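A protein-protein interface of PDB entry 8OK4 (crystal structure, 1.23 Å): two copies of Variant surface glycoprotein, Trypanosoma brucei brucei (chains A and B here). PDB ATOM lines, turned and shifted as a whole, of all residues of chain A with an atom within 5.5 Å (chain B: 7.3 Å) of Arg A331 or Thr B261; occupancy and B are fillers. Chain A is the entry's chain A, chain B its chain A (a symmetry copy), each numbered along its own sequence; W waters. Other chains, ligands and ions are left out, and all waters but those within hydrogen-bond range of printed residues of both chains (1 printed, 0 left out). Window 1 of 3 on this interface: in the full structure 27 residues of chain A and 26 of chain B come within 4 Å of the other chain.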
ATOM      1  N   ALA A 264      11.851 -12.761  -1.877  1.00  0.00           N
ATOM      2  CA  ALA A 264      12.092 -14.195  -1.973  1.00  0.00           C
ATOM      3  C   ALA A 264      12.270 -14.597  -3.426  1.00  0.00           C
ATOM      4  O   ALA A 264      13.138 -15.414  -3.756  1.00  0.00           O
ATOM      5  CB  ALA A 264      10.938 -14.965  -1.328  1.00  0.00           C
ATOM      6  N   ILE A 267      15.823 -13.780  -4.738  1.00  0.00           N
ATOM      7  CA  ILE A 267      16.831 -14.727  -4.283  1.00  0.00           C
ATOM      8  C   ILE A 267      16.641 -16.075  -4.965  1.00  0.00           C
ATOM      9  O   ILE A 267      17.617 -16.710  -5.381  1.00  0.00           O
ATOM     10  CB  ILE A 267      16.762 -14.857  -2.752  1.00  0.00           C
ATOM     11  CG1 ILE A 267      17.038 -13.516  -2.062  1.00  0.00           C
ATOM     12  CG2 ILE A 267      17.733 -15.917  -2.253  1.00  0.00           C
ATOM     13  CD1 ILE A 267      18.426 -12.955  -2.282  1.00  0.00           C
ATOM     14  N   GLU A 268      15.389 -16.543  -5.074  1.00  0.00           N
ATOM     15  CA  GLU A 268      15.122 -17.828  -5.718  1.00  0.00           C
ATOM     16  C   GLU A 268      15.706 -17.865  -7.127  1.00  0.00           C
ATOM     17  O   GLU A 268      16.359 -18.839  -7.523  1.00  0.00           O
ATOM     18  CB  GLU A 268      13.615 -18.120  -5.750  1.00  0.00           C
ATOM     19  CG  GLU A 268      13.284 -19.546  -6.252  1.00  0.00           C
ATOM     20  CD  GLU A 268      13.249 -19.712  -7.784  1.00  0.00           C
ATOM     21  OE1 GLU A 268      13.364 -20.866  -8.277  1.00  0.00           O
ATOM     22  OE2 GLU A 268      13.044 -18.708  -8.496  1.00  0.00           O
ATOM     23  N   LEU A 271      19.517 -18.142  -7.083  1.00  0.00           N
ATOM     24  CA  LEU A 271      20.005 -19.456  -6.677  1.00  0.00           C
ATOM     25  C   LEU A 271      19.738 -20.497  -7.751  1.00  0.00           C
ATOM     26  O   LEU A 271      20.556 -21.397  -7.964  1.00  0.00           O
ATOM     27  CB  LEU A 271      19.382 -19.886  -5.350  1.00  0.00           C
ATOM     28  CG  LEU A 271      19.872 -19.148  -4.105  1.00  0.00           C
ATOM     29  CD1 LEU A 271      18.946 -19.411  -2.924  1.00  0.00           C
ATOM     30  CD2 LEU A 271      21.324 -19.541  -3.798  1.00  0.00           C
ATOM     31  N   LEU A 327      22.066 -18.921   1.760  1.00  0.00           N
ATOM     32  CA  LEU A 327      21.236 -17.988   1.009  1.00  0.00           C
ATOM     33  C   LEU A 327      19.819 -18.507   0.835  1.00  0.00           C
ATOM     34  O   LEU A 327      18.866 -17.716   0.844  1.00  0.00           O
ATOM     35  CB  LEU A 327      21.846 -17.720  -0.357  1.00  0.00           C
ATOM     36  CG  LEU A 327      23.076 -16.837  -0.318  1.00  0.00           C
ATOM     37  CD1 LEU A 327      23.646 -16.760  -1.698  1.00  0.00           C
ATOM     38  CD2 LEU A 327      22.728 -15.455   0.196  1.00  0.00           C
ATOM     39  N   ASP A 328      19.649 -19.825   0.693  1.00  0.00           N
ATOM     40  CA  ASP A 328      18.300 -20.368   0.636  1.00  0.00           C
ATOM     41  C   ASP A 328      17.553 -20.112   1.934  1.00  0.00           C
ATOM     42  O   ASP A 328      16.336 -19.897   1.919  1.00  0.00           O
ATOM     43  CB  ASP A 328      18.322 -21.861   0.325  1.00  0.00           C
ATOM     44  CG  ASP A 328      16.998 -22.349  -0.223  1.00  0.00           C
ATOM     45  OD1 ASP A 328      16.517 -21.758  -1.217  1.00  0.00           O
ATOM     46  OD2 ASP A 328      16.427 -23.297   0.354  1.00  0.00           O
ATOM     47  N   SER A 329      18.267 -20.135   3.059  1.00  0.00           N
ATOM     48  CA  SER A 329      17.649 -19.804   4.337  1.00  0.00           C
ATOM     49  C   SER A 329      17.142 -18.367   4.339  1.00  0.00           C
ATOM     50  O   SER A 329      16.073 -18.077   4.892  1.00  0.00           O
ATOM     51  CB  SER A 329      18.659 -20.039   5.457  1.00  0.00           C
ATOM     52  OG  SER A 329      18.170 -19.556   6.691  1.00  0.00           O
ATOM     53  N   VAL A 330      17.896 -17.456   3.713  1.00  0.00           N
ATOM     54  CA  VAL A 330      17.431 -16.085   3.527  1.00  0.00           C
ATOM     55  C   VAL A 330      16.149 -16.065   2.703  1.00  0.00           C
ATOM     56  O   VAL A 330      15.187 -15.371   3.047  1.00  0.00           O
ATOM     57  CB  VAL A 330      18.539 -15.222   2.893  1.00  0.00           C
ATOM     58  CG1 VAL A 330      17.988 -13.865   2.484  1.00  0.00           C
ATOM     59  CG2 VAL A 330      19.701 -15.053   3.860  1.00  0.00           C
ATOM     60  N   ARG A 331      16.104 -16.836   1.615  1.00  0.00           N
ATOM     61  CA  ARG A 331      14.889 -16.904   0.805  1.00  0.00           C
ATOM     62  C   ARG A 331      13.691 -17.311   1.652  1.00  0.00           C
ATOM     63  O   ARG A 331      12.614 -16.705   1.562  1.00  0.00           O
ATOM     64  CB  ARG A 331      15.080 -17.892  -0.352  1.00  0.00           C
ATOM     65  CG  ARG A 331      13.804 -18.102  -1.197  1.00  0.00           C
ATOM     66  CD  ARG A 331      13.882 -19.313  -2.115  1.00  0.00           C
ATOM     67  NE  ARG A 331      14.101 -20.550  -1.377  1.00  0.00           N
ATOM     68  CZ  ARG A 331      13.149 -21.300  -0.839  1.00  0.00           C
ATOM     69  NH1 ARG A 331      11.875 -20.945  -0.886  1.00  0.00           N
ATOM     70  NH2 ARG A 331      13.484 -22.442  -0.245  1.00  0.00           N
ATOM     71  N   ILE A 332      13.861 -18.349   2.473  1.00  0.00           N
ATOM     72  CA  ILE A 332      12.771 -18.831   3.313  1.00  0.00           C
ATOM     73  C   ILE A 332      12.329 -17.754   4.295  1.00  0.00           C
ATOM     74  O   ILE A 332      11.128 -17.550   4.512  1.00  0.00           O
ATOM     75  CB  ILE A 332      13.186 -20.129   4.029  1.00  0.00           C
ATOM     76  CG1 ILE A 332      13.357 -21.249   3.002  1.00  0.00           C
ATOM     77  CG2 ILE A 332      12.161 -20.478   5.104  1.00  0.00           C
ATOM     78  CD1 ILE A 332      14.162 -22.409   3.509  1.00  0.00           C
ATOM     79  N   LYS A 333      13.287 -17.062   4.920  1.00  0.00           N
ATOM     80  CA  LYS A 333      12.932 -15.992   5.847  1.00  0.00           C
ATOM     81  C   LYS A 333      12.202 -14.864   5.134  1.00  0.00           C
ATOM     82  O   LYS A 333      11.286 -14.255   5.700  1.00  0.00           O
ATOM     83  CB  LYS A 333      14.178 -15.470   6.560  1.00  0.00           C
ATOM     84  CG  LYS A 333      14.773 -16.493   7.496  1.00  0.00           C
ATOM     85  CD  LYS A 333      16.082 -16.032   8.098  1.00  0.00           C
ATOM     86  CE  LYS A 333      16.801 -17.171   8.808  1.00  0.00           C
ATOM     87  NZ  LYS A 333      17.960 -16.672   9.595  1.00  0.00           N
ATOM     88  N   LEU A 334      12.588 -14.573   3.888  1.00  0.00           N
ATOM     89  CA  LEU A 334      11.890 -13.549   3.120  1.00  0.00           C
ATOM     90  C   LEU A 334      10.471 -13.979   2.782  1.00  0.00           C
ATOM     91  O   LEU A 334       9.552 -13.152   2.793  1.00  0.00           O
ATOM     92  CB  LEU A 334      12.671 -13.224   1.850  1.00  0.00           C
ATOM     93  CG  LEU A 334      13.910 -12.363   2.095  1.00  0.00           C
ATOM     94  CD1 LEU A 334      14.764 -12.367   0.835  1.00  0.00           C
ATOM     95  CD2 LEU A 334      13.546 -10.945   2.523  1.00  0.00           C
ATOM     96  N   GLN A 335      10.259 -15.263   2.487  1.00  0.00           N
ATOM     97  CA  GLN A 335       8.896 -15.723   2.247  1.00  0.00           C
ATOM     98  C   GLN A 335       8.032 -15.500   3.480  1.00  0.00           C
ATOM     99  O   GLN A 335       6.884 -15.049   3.381  1.00  0.00           O
ATOM    100  CB  GLN A 335       8.878 -17.200   1.865  1.00  0.00           C
ATOM    101  CG  GLN A 335       9.407 -17.486   0.480  1.00  0.00           C
ATOM    102  CD  GLN A 335       9.374 -18.962   0.147  1.00  0.00           C
ATOM    103  OE1 GLN A 335       9.217 -19.808   1.032  1.00  0.00           O
ATOM    104  NE2 GLN A 335       9.529 -19.285  -1.133  1.00  0.00           N
ATOM    105  N   LYS A 336       8.571 -15.818   4.659  1.00  0.00           N
ATOM    106  CA  LYS A 336       7.822 -15.605   5.891  1.00  0.00           C
ATOM    107  C   LYS A 336       7.567 -14.123   6.133  1.00  0.00           C
ATOM    108  O   LYS A 336       6.471 -13.736   6.552  1.00  0.00           O
ATOM    109  CB  LYS A 336       8.573 -16.220   7.071  1.00  0.00           C
ATOM    110  CG  LYS A 336       8.849 -17.710   6.936  1.00  0.00           C
ATOM    111  CD  LYS A 336       7.575 -18.517   6.720  1.00  0.00           C
ATOM    112  CE  LYS A 336       7.871 -20.008   6.597  1.00  0.00           C
ATOM    113  NZ  LYS A 336       6.815 -20.851   7.230  1.00  0.00           N
ATOM    114  N   LEU B  20      11.531 -29.768 -11.548  1.00  0.00           N
ATOM    115  CA  LEU B  20      10.196 -29.580 -10.995  1.00  0.00           C
ATOM    116  C   LEU B  20       9.357 -30.849 -10.978  1.00  0.00           C
ATOM    117  O   LEU B  20       8.290 -30.850 -10.353  1.00  0.00           O
ATOM    118  CB  LEU B  20       9.426 -28.559 -11.836  1.00  0.00           C
ATOM    119  CG  LEU B  20      10.059 -27.180 -11.977  1.00  0.00           C
ATOM    120  CD1 LEU B  20       9.265 -26.307 -12.941  1.00  0.00           C
ATOM    121  CD2 LEU B  20      10.168 -26.527 -10.622  1.00  0.00           C
ATOM    122  N   ARG B  24       8.708 -33.345  -6.628  1.00  0.00           N
ATOM    123  CA  ARG B  24       9.653 -32.386  -6.076  1.00  0.00           C
ATOM    124  C   ARG B  24       9.067 -30.989  -5.939  1.00  0.00           C
ATOM    125  O   ARG B  24       9.545 -30.217  -5.100  1.00  0.00           O
ATOM    126  CB  ARG B  24      10.917 -32.358  -6.942  1.00  0.00           C
ATOM    127  CG  ARG B  24      11.684 -33.680  -6.924  1.00  0.00           C
ATOM    128  CD  ARG B  24      13.018 -33.580  -7.662  1.00  0.00           C
ATOM    129  NE  ARG B  24      12.833 -33.556  -9.109  1.00  0.00           N
ATOM    130  CZ  ARG B  24      12.532 -34.618  -9.846  1.00  0.00           C
ATOM    131  NH1 ARG B  24      12.402 -35.817  -9.306  1.00  0.00           N
ATOM    132  NH2 ARG B  24      12.382 -34.475 -11.163  1.00  0.00           N
ATOM    133  N   ALA B  25       8.038 -30.654  -6.717  1.00  0.00           N
ATOM    134  CA  ALA B  25       7.426 -29.330  -6.677  1.00  0.00           C
ATOM    135  C   ALA B  25       6.437 -29.261  -5.520  1.00  0.00           C
ATOM    136  O   ALA B  25       5.495 -30.059  -5.457  1.00  0.00           O
ATOM    137  CB  ALA B  25       6.723 -29.052  -8.006  1.00  0.00           C
ATOM    138  N   LYS B  26       6.650 -28.309  -4.605  1.00  0.00           N
ATOM    139  CA  LYS B  26       5.867 -28.197  -3.380  1.00  0.00           C
ATOM    140  C   LYS B  26       5.335 -26.779  -3.177  1.00  0.00           C
ATOM    141  O   LYS B  26       6.066 -25.799  -3.339  1.00  0.00           O
ATOM    142  CB  LYS B  26       6.722 -28.554  -2.152  1.00  0.00           C
ATOM    143  CG  LYS B  26       7.475 -29.874  -2.237  1.00  0.00           C
ATOM    144  CD  LYS B  26       6.527 -31.059  -2.257  1.00  0.00           C
ATOM    145  CE  LYS B  26       7.076 -32.239  -1.469  1.00  0.00           C
ATOM    146  NZ  LYS B  26       8.133 -32.977  -2.210  1.00  0.00           N
ATOM    147  N   LEU B  27       4.081 -26.671  -2.749  1.00  0.00           N
ATOM    148  CA  LEU B  27       3.479 -25.361  -2.530  1.00  0.00           C
ATOM    149  C   LEU B  27       4.067 -24.678  -1.295  1.00  0.00           C
ATOM    150  O   LEU B  27       4.217 -25.300  -0.239  1.00  0.00           O
ATOM    151  CB  LEU B  27       1.972 -25.524  -2.345  1.00  0.00           C
ATOM    152  CG  LEU B  27       1.155 -25.548  -3.637  1.00  0.00           C
ATOM    153  CD1 LEU B  27      -0.252 -26.058  -3.391  1.00  0.00           C
ATOM    154  CD2 LEU B  27       1.117 -24.160  -4.259  1.00  0.00           C
ATOM    155  N   GLU B  28       4.391 -23.378  -1.426  1.00  0.00           N
ATOM    156  CA  GLU B  28       4.879 -22.623  -0.273  1.00  0.00           C
ATOM    157  C   GLU B  28       3.903 -22.710   0.894  1.00  0.00           C
ATOM    158  O   GLU B  28       4.309 -22.778   2.060  1.00  0.00           O
ATOM    159  CB  GLU B  28       5.061 -21.124  -0.574  1.00  0.00           C
ATOM    160  CG  GLU B  28       5.650 -20.705  -1.910  1.00  0.00           C
ATOM    161  CD  GLU B  28       5.180 -19.317  -2.346  1.00  0.00           C
ATOM    162  OE1 GLU B  28       3.975 -19.015  -2.211  1.00  0.00           O
ATOM    163  OE2 GLU B  28       6.023 -18.522  -2.815  1.00  0.00           O
ATOM    164  N   THR B  29       2.608 -22.680   0.593  1.00  0.00           N
ATOM    165  CA  THR B  29       1.600 -22.352   1.589  1.00  0.00           C
ATOM    166  C   THR B  29       0.290 -23.008   1.195  1.00  0.00           C
ATOM    167  O   THR B  29      -0.113 -22.936   0.032  1.00  0.00           O
ATOM    168  CB  THR B  29       1.407 -20.831   1.635  1.00  0.00           C
ATOM    169  OG1 THR B  29       2.662 -20.190   1.893  1.00  0.00           O
ATOM    170  CG2 THR B  29       0.408 -20.448   2.707  1.00  0.00           C
ATOM    171  N   LYS B 259      13.814 -30.707  -3.516  1.00  0.00           N
ATOM    172  CA  LYS B 259      12.465 -30.182  -3.694  1.00  0.00           C
ATOM    173  C   LYS B 259      12.555 -28.743  -4.184  1.00  0.00           C
ATOM    174  O   LYS B 259      13.593 -28.088  -4.062  1.00  0.00           O
ATOM    175  CB  LYS B 259      11.666 -30.241  -2.380  1.00  0.00           C
ATOM    176  N   THR B 260      11.448 -28.266  -4.759  1.00  0.00           N
ATOM    177  CA  THR B 260      11.307 -26.894  -5.224  1.00  0.00           C
ATOM    178  C   THR B 260      10.013 -26.339  -4.666  1.00  0.00           C
ATOM    179  O   THR B 260       8.973 -26.998  -4.756  1.00  0.00           O
ATOM    180  CB  THR B 260      11.201 -26.834  -6.746  1.00  0.00           C
ATOM    181  OG1 THR B 260      12.451 -27.207  -7.314  1.00  0.00           O
ATOM    182  CG2 THR B 260      10.852 -25.431  -7.219  1.00  0.00           C
ATOM    183  N   THR B 261      10.068 -25.129  -4.119  1.00  0.00           N
ATOM    184  CA  THR B 261       8.873 -24.451  -3.631  1.00  0.00           C
ATOM    185  C   THR B 261       8.150 -23.839  -4.826  1.00  0.00           C
ATOM    186  O   THR B 261       8.661 -22.916  -5.467  1.00  0.00           O
ATOM    187  CB  THR B 261       9.259 -23.389  -2.608  1.00  0.00           C
ATOM    188  OG1 THR B 261       9.948 -24.004  -1.511  1.00  0.00           O
ATOM    189  CG2 THR B 261       8.036 -22.705  -2.079  1.00  0.00           C
ATOM    190  N   LEU B 262       6.964 -24.353  -5.130  1.00  0.00           N
ATOM    191  CA  LEU B 262       6.213 -23.884  -6.284  1.00  0.00           C
ATOM    192  C   LEU B 262       5.708 -22.472  -6.036  1.00  0.00           C
ATOM    193  O   LEU B 262       4.952 -22.228  -5.087  1.00  0.00           O
ATOM    194  CB  LEU B 262       5.011 -24.787  -6.519  1.00  0.00           C
ATOM    195  CG  LEU B 262       5.179 -26.024  -7.383  1.00  0.00           C
ATOM    196  CD1 LEU B 262       3.860 -26.777  -7.414  1.00  0.00           C
ATOM    197  CD2 LEU B 262       5.636 -25.643  -8.781  1.00  0.00           C
ATOM    198  N   SER B 263       6.097 -21.549  -6.906  1.00  0.00           N
ATOM    199  CA  SER B 263       5.503 -20.226  -6.936  1.00  0.00           C
ATOM    200  C   SER B 263       5.340 -19.825  -8.393  1.00  0.00           C
ATOM    201  O   SER B 263       6.042 -20.321  -9.277  1.00  0.00           O
ATOM    202  CB  SER B 263       6.347 -19.195  -6.180  1.00  0.00           C
ATOM    203  OG  SER B 263       7.541 -18.908  -6.887  1.00  0.00           O
ATOM    204  N   ALA B 264       4.410 -18.909  -8.642  1.00  0.00           N
ATOM    205  CA  ALA B 264       4.189 -18.458 -10.010  1.00  0.00           C
ATOM    206  C   ALA B 264       5.447 -17.796 -10.548  1.00  0.00           C
ATOM    207  O   ALA B 264       5.822 -18.000 -11.710  1.00  0.00           O
ATOM    208  CB  ALA B 264       3.000 -17.498 -10.061  1.00  0.00           C
ATOM    209  N   ALA B 266       8.546 -18.428  -9.746  1.00  0.00           N
ATOM    210  CA  ALA B 266       9.588 -19.408 -10.036  1.00  0.00           C
ATOM    211  C   ALA B 266       9.342 -20.102 -11.372  1.00  0.00           C
ATOM    212  O   ALA B 266      10.287 -20.376 -12.121  1.00  0.00           O
ATOM    213  CB  ALA B 266       9.659 -20.427  -8.903  1.00  0.00           C
ATOM    214  N   ILE B 267       8.085 -20.393 -11.691  1.00  0.00           N
ATOM    215  CA  ILE B 267       7.771 -20.998 -12.978  1.00  0.00           C
ATOM    216  C   ILE B 267       7.949 -19.984 -14.099  1.00  0.00           C
ATOM    217  O   ILE B 267       8.491 -20.312 -15.161  1.00  0.00           O
ATOM    218  CB  ILE B 267       6.339 -21.557 -12.949  1.00  0.00           C
ATOM    219  CG1 ILE B 267       6.181 -22.640 -11.875  1.00  0.00           C
ATOM    220  CG2 ILE B 267       5.942 -22.104 -14.312  1.00  0.00           C
ATOM    221  CD1 ILE B 267       7.015 -23.883 -12.091  1.00  0.00           C
ATOM    222  N   ARG B 270      11.579 -19.645 -15.118  1.00  0.00           N
ATOM    223  CA  ARG B 270      12.076 -20.813 -15.832  1.00  0.00           C
ATOM    224  C   ARG B 270      11.557 -20.853 -17.262  1.00  0.00           C
ATOM    225  O   ARG B 270      12.291 -21.227 -18.189  1.00  0.00           O
ATOM    226  CB  ARG B 270      11.658 -22.070 -15.080  1.00  0.00           C
ATOM    227  CG  ARG B 270      12.505 -22.345 -13.864  1.00  0.00           C
ATOM    228  CD  ARG B 270      11.833 -23.408 -13.030  1.00  0.00           C
ATOM    229  NE  ARG B 270      12.713 -23.943 -12.003  1.00  0.00           N
ATOM    230  CZ  ARG B 270      12.906 -23.379 -10.821  1.00  0.00           C
ATOM    231  NH1 ARG B 270      12.343 -22.225 -10.508  1.00  0.00           N
ATOM    232  NH2 ARG B 270      13.684 -23.986  -9.932  1.00  0.00           N
ATOM    233  N   LEU B 334      -0.996 -21.255 -10.171  1.00  0.00           N
ATOM    234  CA  LEU B 334      -0.272 -20.792  -8.994  1.00  0.00           C
ATOM    235  C   LEU B 334      -0.581 -19.335  -8.687  1.00  0.00           C
ATOM    236  O   LEU B 334      -0.687 -18.955  -7.516  1.00  0.00           O
ATOM    237  CB  LEU B 334       1.228 -20.996  -9.187  1.00  0.00           C
ATOM    238  CG  LEU B 334       1.674 -22.450  -9.038  1.00  0.00           C
ATOM    239  CD1 LEU B 334       3.102 -22.577  -9.551  1.00  0.00           C
ATOM    240  CD2 LEU B 334       1.550 -22.942  -7.598  1.00  0.00           C
HETATM  241  O   HOH W   1      13.022 -19.054 -11.467  1.00  0.00           O
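3 positions are printed for both chains.
Of the 5 pairs that touch across the chains among the printed residues, none has its exchanged pair printed and touching as well.
OE1 of Glu A268 touches CB of Ala B266 (3.8 Å).
Thr B261 touches Arg A331 (OG1 to NH1, 3.7 Å).
Gln A335 touches Glu B28.
Thr B261 touches Gln A335 (CG2 to NE2, 3.8 Å).
Water W1 lies within hydrogen-bond range of the side-chain carboxylate (OE2) of Glu A268 (3.0 Å), the backbone carbonyl oxygen (O) of Ala B266 (3.1 Å) and the guanidinium group (NH1) of Arg B270 (3.4 Å).
Printed residues of chain B within 4 Å of Glu A268: Ala B266 (3.8 Å) and Arg B270 (2.8 Å).
Of chain B, only Thr B261 (3.7 Å) comes within 4 Å of Arg A331.
Of the printed residues of chain B, Gln A335 touches Glu B28 and Thr B261.
Printed residues of chain A within 4 Å of Glu B28: Gln A335 (3.96 Å).
Printed residues of chain A within 4 Å of Thr B261: Arg A331 and Gln A335.
Of the printed residues of chain A, Ala B266 touches Glu A268.
Of the printed residues of chain A, Arg B270 touches Glu A268 (2.8 Å).
The nearest printed residue of chain A that does not touch Glu B28 is Lys A336 (6.1 Å).
Printed residues of chain A that touch a printed residue of chain B: Glu A268, Arg A331 and Gln A335.
Of the 17 printed residues of chain B, 4 touch a printed residue of chain A.
Printed residues of chain B that touch a printed residue of chain A: Glu B28, Thr B261, Ala B266 and Arg B270.
Hydrophobic or aromatic side chains of chain B within 4 Å of the printed part of chain A: Ala B266.
Among the printed residues, Asp or Glu carboxylates within 4 Å of a Lys or Arg side-chain nitrogen of the other chain: Glu A268 with Arg B270 (2.8 Å).
The side-chain amide nitrogen (NE2) of Gln A335 lies close to the guanidinium group (NH1) of Arg A331.
The side-chain carboxylate of Asp A328 lies within salt-bridge range of the guanidinium group of Arg A331.
The guanidinium group (NH1) of Arg B270 lies within hydrogen-bond range of the backbone carbonyl oxygen (O) of Ala B266 (3.2 Å).
The side-chain hydroxyl (OG) of Ser B263 is in hydrogen-bond range of the backbone NH (N) of Ala B266 (3.1 Å).
The guanidinium group (NH1) of Arg B270 is in salt-bridge range of the side-chain carboxylate (OE1) of Glu A268.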
